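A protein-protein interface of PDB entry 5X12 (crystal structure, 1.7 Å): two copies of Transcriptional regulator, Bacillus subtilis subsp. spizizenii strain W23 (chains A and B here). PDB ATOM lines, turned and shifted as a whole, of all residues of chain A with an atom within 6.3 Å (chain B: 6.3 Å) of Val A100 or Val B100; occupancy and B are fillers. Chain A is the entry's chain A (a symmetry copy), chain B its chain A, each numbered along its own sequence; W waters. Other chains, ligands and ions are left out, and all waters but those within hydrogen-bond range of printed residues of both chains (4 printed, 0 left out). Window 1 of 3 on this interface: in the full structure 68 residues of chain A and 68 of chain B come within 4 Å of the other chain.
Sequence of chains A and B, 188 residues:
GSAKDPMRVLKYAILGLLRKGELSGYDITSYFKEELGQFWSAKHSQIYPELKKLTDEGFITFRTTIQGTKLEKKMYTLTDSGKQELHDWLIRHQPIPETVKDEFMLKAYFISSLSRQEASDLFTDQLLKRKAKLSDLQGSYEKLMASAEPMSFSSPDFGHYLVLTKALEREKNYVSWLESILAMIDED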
ATOM      1  N   GLN A  38       9.056   0.658 -20.442  1.00  0.00           N
ATOM      2  CA  GLN A  38      10.161   0.506 -19.518  1.00  0.00           C
ATOM      3  C   GLN A  38       9.708   0.646 -18.058  1.00  0.00           C
ATOM      4  O   GLN A  38      10.327   0.058 -17.173  1.00  0.00           O
ATOM      5  CB  GLN A  38      11.262   1.535 -19.841  1.00  0.00           C
ATOM      6  CG  GLN A  38      11.862   1.367 -21.234  1.00  0.00           C
ATOM      7  CD  GLN A  38      12.639   0.073 -21.386  1.00  0.00           C
ATOM      8  OE1 GLN A  38      13.698  -0.107 -20.776  1.00  0.00           O
ATOM      9  NE2 GLN A  38      12.118  -0.840 -22.210  1.00  0.00           N
ATOM     10  N   PHE A  39       8.669   1.445 -17.805  1.00  0.00           N
ATOM     11  CA  PHE A  39       8.101   1.578 -16.444  1.00  0.00           C
ATOM     12  C   PHE A  39       6.613   1.180 -16.383  1.00  0.00           C
ATOM     13  O   PHE A  39       6.075   0.969 -15.295  1.00  0.00           O
ATOM     14  CB  PHE A  39       8.314   3.006 -15.884  1.00  0.00           C
ATOM     15  CG  PHE A  39       7.464   4.074 -16.554  1.00  0.00           C
ATOM     16  CD1 PHE A  39       7.843   4.621 -17.766  1.00  0.00           C
ATOM     17  CD2 PHE A  39       6.284   4.534 -15.962  1.00  0.00           C
ATOM     18  CE1 PHE A  39       7.044   5.581 -18.389  1.00  0.00           C
ATOM     19  CE2 PHE A  39       5.509   5.481 -16.569  1.00  0.00           C
ATOM     20  CZ  PHE A  39       5.894   6.005 -17.791  1.00  0.00           C
ATOM     21  N   PRO A  97       1.557   2.215  -2.279  1.00  0.00           N
ATOM     22  CA  PRO A  97       1.408   0.785  -2.419  1.00  0.00           C
ATOM     23  C   PRO A  97       2.423   0.014  -1.555  1.00  0.00           C
ATOM     24  O   PRO A  97       3.419   0.580  -1.063  1.00  0.00           O
ATOM     25  CB  PRO A  97       1.642   0.569  -3.926  1.00  0.00           C
ATOM     26  CG  PRO A  97       2.647   1.622  -4.297  1.00  0.00           C
ATOM     27  CD  PRO A  97       2.286   2.826  -3.418  1.00  0.00           C
ATOM     28  N   GLU A  98       2.154  -1.274  -1.368  1.00  0.00           N
ATOM     29  CA  GLU A  98       3.067  -2.155  -0.628  1.00  0.00           C
ATOM     30  C   GLU A  98       4.361  -2.287  -1.414  1.00  0.00           C
ATOM     31  O   GLU A  98       4.405  -2.079  -2.642  1.00  0.00           O
ATOM     32  CB  GLU A  98       2.431  -3.534  -0.384  1.00  0.00           C
ATOM     33  N   THR A  99       5.424  -2.597  -0.689  1.00  0.00           N
ATOM     34  CA  THR A  99       6.740  -2.770  -1.275  1.00  0.00           C
ATOM     35  C   THR A  99       6.698  -3.865  -2.326  1.00  0.00           C
ATOM     36  O   THR A  99       6.100  -4.927  -2.101  1.00  0.00           O
ATOM     37  CB  THR A  99       7.756  -3.099  -0.150  1.00  0.00           C
ATOM     38  OG1 THR A  99       7.825  -1.973   0.756  1.00  0.00           O
ATOM     39  CG2 THR A  99       9.147  -3.418  -0.715  1.00  0.00           C
ATOM     40  N   VAL A 100       7.319  -3.611  -3.473  1.00  0.00           N
ATOM     41  CA  VAL A 100       7.306  -4.602  -4.570  1.00  0.00           C
ATOM     42  C   VAL A 100       8.333  -5.679  -4.214  1.00  0.00           C
ATOM     43  O   VAL A 100       9.369  -5.342  -3.636  1.00  0.00           O
ATOM     44  CB  VAL A 100       7.625  -3.933  -5.930  1.00  0.00           C
ATOM     45  N   LYS A 101       8.035  -6.961  -4.465  1.00  0.00           N
ATOM     46  CA  LYS A 101       8.991  -8.039  -4.125  1.00  0.00           C
ATOM     47  C   LYS A 101      10.303  -7.908  -4.920  1.00  0.00           C
ATOM     48  O   LYS A 101      10.282  -7.892  -6.159  1.00  0.00           O
ATOM     49  CB  LYS A 101       8.384  -9.435  -4.354  1.00  0.00           C
ATOM     50  CG  LYS A 101       7.433  -9.868  -3.255  1.00  0.00           C
ATOM     51  CD  LYS A 101       6.679 -11.186  -3.625  1.00  0.00           C
ATOM     52  CE  LYS A 101       5.966 -11.760  -2.436  1.00  0.00           C
ATOM     53  NZ  LYS A 101       4.858 -10.811  -1.977  1.00  0.00           N
ATOM     54  N   ASP A 102      11.424  -7.829  -4.209  1.00  0.00           N
ATOM     55  CA  ASP A 102      12.759  -7.750  -4.836  1.00  0.00           C
ATOM     56  C   ASP A 102      13.478  -9.013  -4.411  1.00  0.00           C
ATOM     57  O   ASP A 102      13.834  -9.152  -3.246  1.00  0.00           O
ATOM     58  CB  ASP A 102      13.493  -6.486  -4.361  1.00  0.00           C
ATOM     59  CG  ASP A 102      14.862  -6.312  -4.999  1.00  0.00           C
ATOM     60  OD1 ASP A 102      15.440  -7.320  -5.413  1.00  0.00           O
ATOM     61  OD2 ASP A 102      15.352  -5.159  -5.101  1.00  0.00           O
ATOM     62  N   ARG A 170      16.728   6.225  -8.631  1.00  0.00           N
ATOM     63  CA  ARG A 170      16.495   4.917  -8.017  1.00  0.00           C
ATOM     64  C   ARG A 170      17.726   4.005  -8.215  1.00  0.00           C
ATOM     65  O   ARG A 170      18.161   3.280  -7.274  1.00  0.00           O
ATOM     66  CB  ARG A 170      15.257   4.259  -8.604  1.00  0.00           C
ATOM     67  CG  ARG A 170      15.026   2.865  -8.161  1.00  0.00           C
ATOM     68  CD  ARG A 170      13.694   2.257  -8.764  1.00  0.00           C
ATOM     69  NE  ARG A 170      13.653   2.120 -10.212  1.00  0.00           N
ATOM     70  CZ  ARG A 170      12.859   2.813 -11.041  1.00  0.00           C
ATOM     71  NH1 ARG A 170      12.071   3.812 -10.612  1.00  0.00           N
ATOM     72  NH2 ARG A 170      12.908   2.550 -12.330  1.00  0.00           N
ATOM     73  N   GLN B  38       6.626  -7.212   5.157  1.00  0.00           N
ATOM     74  CA  GLN B  38       6.777  -5.836   4.728  1.00  0.00           C
ATOM     75  C   GLN B  38       7.475  -5.737   3.365  1.00  0.00           C
ATOM     76  O   GLN B  38       7.233  -4.783   2.628  1.00  0.00           O
ATOM     77  CB  GLN B  38       7.553  -5.036   5.792  1.00  0.00           C
ATOM     78  CG  GLN B  38       6.846  -4.973   7.143  1.00  0.00           C
ATOM     79  CD  GLN B  38       5.552  -4.182   7.091  1.00  0.00           C
ATOM     80  OE1 GLN B  38       5.561  -2.961   6.902  1.00  0.00           O
ATOM     81  NE2 GLN B  38       4.424  -4.875   7.264  1.00  0.00           N
ATOM     82  N   PHE B  39       8.361  -6.685   3.051  1.00  0.00           N
ATOM     83  CA  PHE B  39       9.023  -6.726   1.728  1.00  0.00           C
ATOM     84  C   PHE B  39       8.751  -8.043   0.973  1.00  0.00           C
ATOM     85  O   PHE B  39       8.990  -8.122  -0.233  1.00  0.00           O
ATOM     86  CB  PHE B  39      10.545  -6.466   1.852  1.00  0.00           C
ATOM     87  CG  PHE B  39      11.324  -7.602   2.495  1.00  0.00           C
ATOM     88  CD1 PHE B  39      11.357  -7.748   3.869  1.00  0.00           C
ATOM     89  CD2 PHE B  39      12.031  -8.523   1.715  1.00  0.00           C
ATOM     90  CE1 PHE B  39      12.052  -8.809   4.450  1.00  0.00           C
ATOM     91  CE2 PHE B  39      12.718  -9.556   2.288  1.00  0.00           C
ATOM     92  CZ  PHE B  39      12.726  -9.697   3.664  1.00  0.00           C
ATOM     93  N   PRO B  97      15.247  -7.676 -12.563  1.00  0.00           N
ATOM     94  CA  PRO B  97      13.877  -7.724 -13.022  1.00  0.00           C
ATOM     95  C   PRO B  97      13.438  -6.393 -13.660  1.00  0.00           C
ATOM     96  O   PRO B  97      14.097  -5.347 -13.499  1.00  0.00           O
ATOM     97  CB  PRO B  97      13.101  -8.037 -11.729  1.00  0.00           C
ATOM     98  CG  PRO B  97      13.887  -7.345 -10.652  1.00  0.00           C
ATOM     99  CD  PRO B  97      15.350  -7.477 -11.097  1.00  0.00           C
ATOM    100  N   GLU B  98      12.329  -6.448 -14.390  1.00  0.00           N
ATOM    101  CA  GLU B  98      11.745  -5.246 -15.000  1.00  0.00           C
ATOM    102  C   GLU B  98      11.265  -4.322 -13.893  1.00  0.00           C
ATOM    103  O   GLU B  98      10.994  -4.750 -12.754  1.00  0.00           O
ATOM    104  CB  GLU B  98      10.591  -5.610 -15.950  1.00  0.00           C
ATOM    105  N   THR B  99      11.197  -3.042 -14.226  1.00  0.00           N
ATOM    106  CA  THR B  99      10.751  -2.021 -13.296  1.00  0.00           C
ATOM    107  C   THR B  99       9.346  -2.335 -12.816  1.00  0.00           C
ATOM    108  O   THR B  99       8.477  -2.702 -13.620  1.00  0.00           O
ATOM    109  CB  THR B  99      10.818  -0.637 -13.995  1.00  0.00           C
ATOM    110  OG1 THR B  99      12.197  -0.353 -14.329  1.00  0.00           O
ATOM    111  CG2 THR B  99      10.242   0.476 -13.107  1.00  0.00           C
ATOM    112  N   VAL B 100       9.120  -2.205 -11.514  1.00  0.00           N
ATOM    113  CA  VAL B 100       7.792  -2.519 -10.945  1.00  0.00           C
ATOM    114  C   VAL B 100       6.877  -1.333 -11.257  1.00  0.00           C
ATOM    115  O   VAL B 100       7.355  -0.196 -11.238  1.00  0.00           O
ATOM    116  CB  VAL B 100       7.886  -2.787  -9.423  1.00  0.00           C
ATOM    117  N   LYS B 101       5.611  -1.575 -11.622  1.00  0.00           N
ATOM    118  CA  LYS B 101       4.694  -0.459 -11.947  1.00  0.00           C
ATOM    119  C   LYS B 101       4.452   0.452 -10.730  1.00  0.00           C
ATOM    120  O   LYS B 101       4.003  -0.022  -9.677  1.00  0.00           O
ATOM    121  CB  LYS B 101       3.345  -0.968 -12.490  1.00  0.00           C
ATOM    122  CG  LYS B 101       3.404  -1.405 -13.940  1.00  0.00           C
ATOM    123  CD  LYS B 101       2.082  -2.108 -14.389  1.00  0.00           C
ATOM    124  CE  LYS B 101       2.031  -2.277 -15.879  1.00  0.00           C
ATOM    125  NZ  LYS B 101       3.137  -3.229 -16.339  1.00  0.00           N
ATOM    126  N   ASP B 102       4.736   1.742 -10.887  1.00  0.00           N
ATOM    127  CA  ASP B 102       4.509   2.740  -9.824  1.00  0.00           C
ATOM    128  C   ASP B 102       3.463   3.686 -10.378  1.00  0.00           C
ATOM    129  O   ASP B 102       3.753   4.454 -11.288  1.00  0.00           O
ATOM    130  CB  ASP B 102       5.820   3.470  -9.492  1.00  0.00           C
ATOM    131  CG  ASP B 102       5.674   4.487  -8.372  1.00  0.00           C
ATOM    132  OD1 ASP B 102       4.557   4.970  -8.170  1.00  0.00           O
ATOM    133  OD2 ASP B 102       6.679   4.790  -7.680  1.00  0.00           O
ATOM    134  N   ARG B 170      15.826   3.656   0.000  1.00  0.00           N
ATOM    135  CA  ARG B 170      14.857   3.793  -1.087  1.00  0.00           C
ATOM    136  C   ARG B 170      13.877   4.950  -0.791  1.00  0.00           C
ATOM    137  O   ARG B 170      13.538   5.767  -1.694  1.00  0.00           O
ATOM    138  CB  ARG B 170      14.089   2.497  -1.292  1.00  0.00           C
ATOM    139  CG  ARG B 170      12.976   2.581  -2.265  1.00  0.00           C
ATOM    140  CD  ARG B 170      12.253   1.189  -2.472  1.00  0.00           C
ATOM    141  NE  ARG B 170      11.586   0.635  -1.304  1.00  0.00           N
ATOM    142  CZ  ARG B 170      11.956  -0.470  -0.642  1.00  0.00           C
ATOM    143  NH1 ARG B 170      13.080  -1.142  -0.938  1.00  0.00           N
ATOM    144  NH2 ARG B 170      11.227  -0.870   0.378  1.00  0.00           N
HETATM  145  O   HOH W   1       6.491   2.298 -12.957  1.00  0.00           O
HETATM  146  O   HOH W   2       5.969  -2.130 -16.054  1.00  0.00           O
HETATM  147  O   HOH W   3       5.842  -8.193  -0.757  1.00  0.00           O
HETATM  148  O   HOH W   4      11.077  -7.015  -1.584  1.00  0.00           O
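O of Phe A39 touches CG of Lys B101, at 3.8 Å. Thr A99 touches Arg B170. Val A100 touches Val B100. Lys A101 touches Phe B39. Arg A170 touches Thr B99.
The backbone carbonyl oxygen (O) of Gln B38 sits close to the side-chain hydroxyl (OG1) of Thr A99, 3.4 Å away. The backbone carbonyl oxygen of Gln A38 lies close to the side-chain hydroxyl of Thr B99 (3.4 Å).
Water W4 lies within hydrogen-bond range of O of Phe B39 (2.7 Å), N of Asp A102 (2.8 Å) and O of Val A100 (3.2 Å). Water W1 lies within hydrogen-bond range of O of Phe A39 (2.7 Å), N of Asp B102 (2.8 Å) and O of Val B100 (3.1 Å). Water W3 lies within hydrogen-bond range of the side-chain amino group of Lys A101 and the backbone carbonyl oxygen of Phe B39. Water W2 bridges the side-chain amino group (NZ) of Lys B101 and the backbone carbonyl oxygen (O) of Phe A39.
Val A100 touches just one residue of chain B: Val B100. Val B100 touches just one residue of chain A: Val A100. Printed residues of chain B within 4 Å of Gln A38: Thr B99. Printed residues of chain A within 4 Å of Gln B38: Thr A99 (3.3 Å). Of the printed residues of chain A, Phe B39 touches Lys A101.
Of the 9 printed residues of chain B, 6 touch a printed residue of chain A. Hydrophobic or aromatic side chains of chain A that line the printed part of chain B: Val A100. Among the printed residues, 7 pairs touch across the chains. Among the printed residues, no Asp or Glu carboxylate lies within 4 Å of a Lys or Arg side-chain nitrogen of the other chain.
Gln A38 touches Thr B99, and with the chains exchanged Thr A99 touches Gln B38. Phe A39 touches Lys B101, and with the chains exchanged Lys A101 touches Phe B39. Thr A99 touches Arg B170, and with the chains exchanged Arg A170 touches Thr B99. Val B100 touches its own counterpart, Val A100. 9 positions are printed for both chains. Of the 7 pairs that touch across the chains among the printed residues, 7 have their exchanged pair printed and touching as well.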
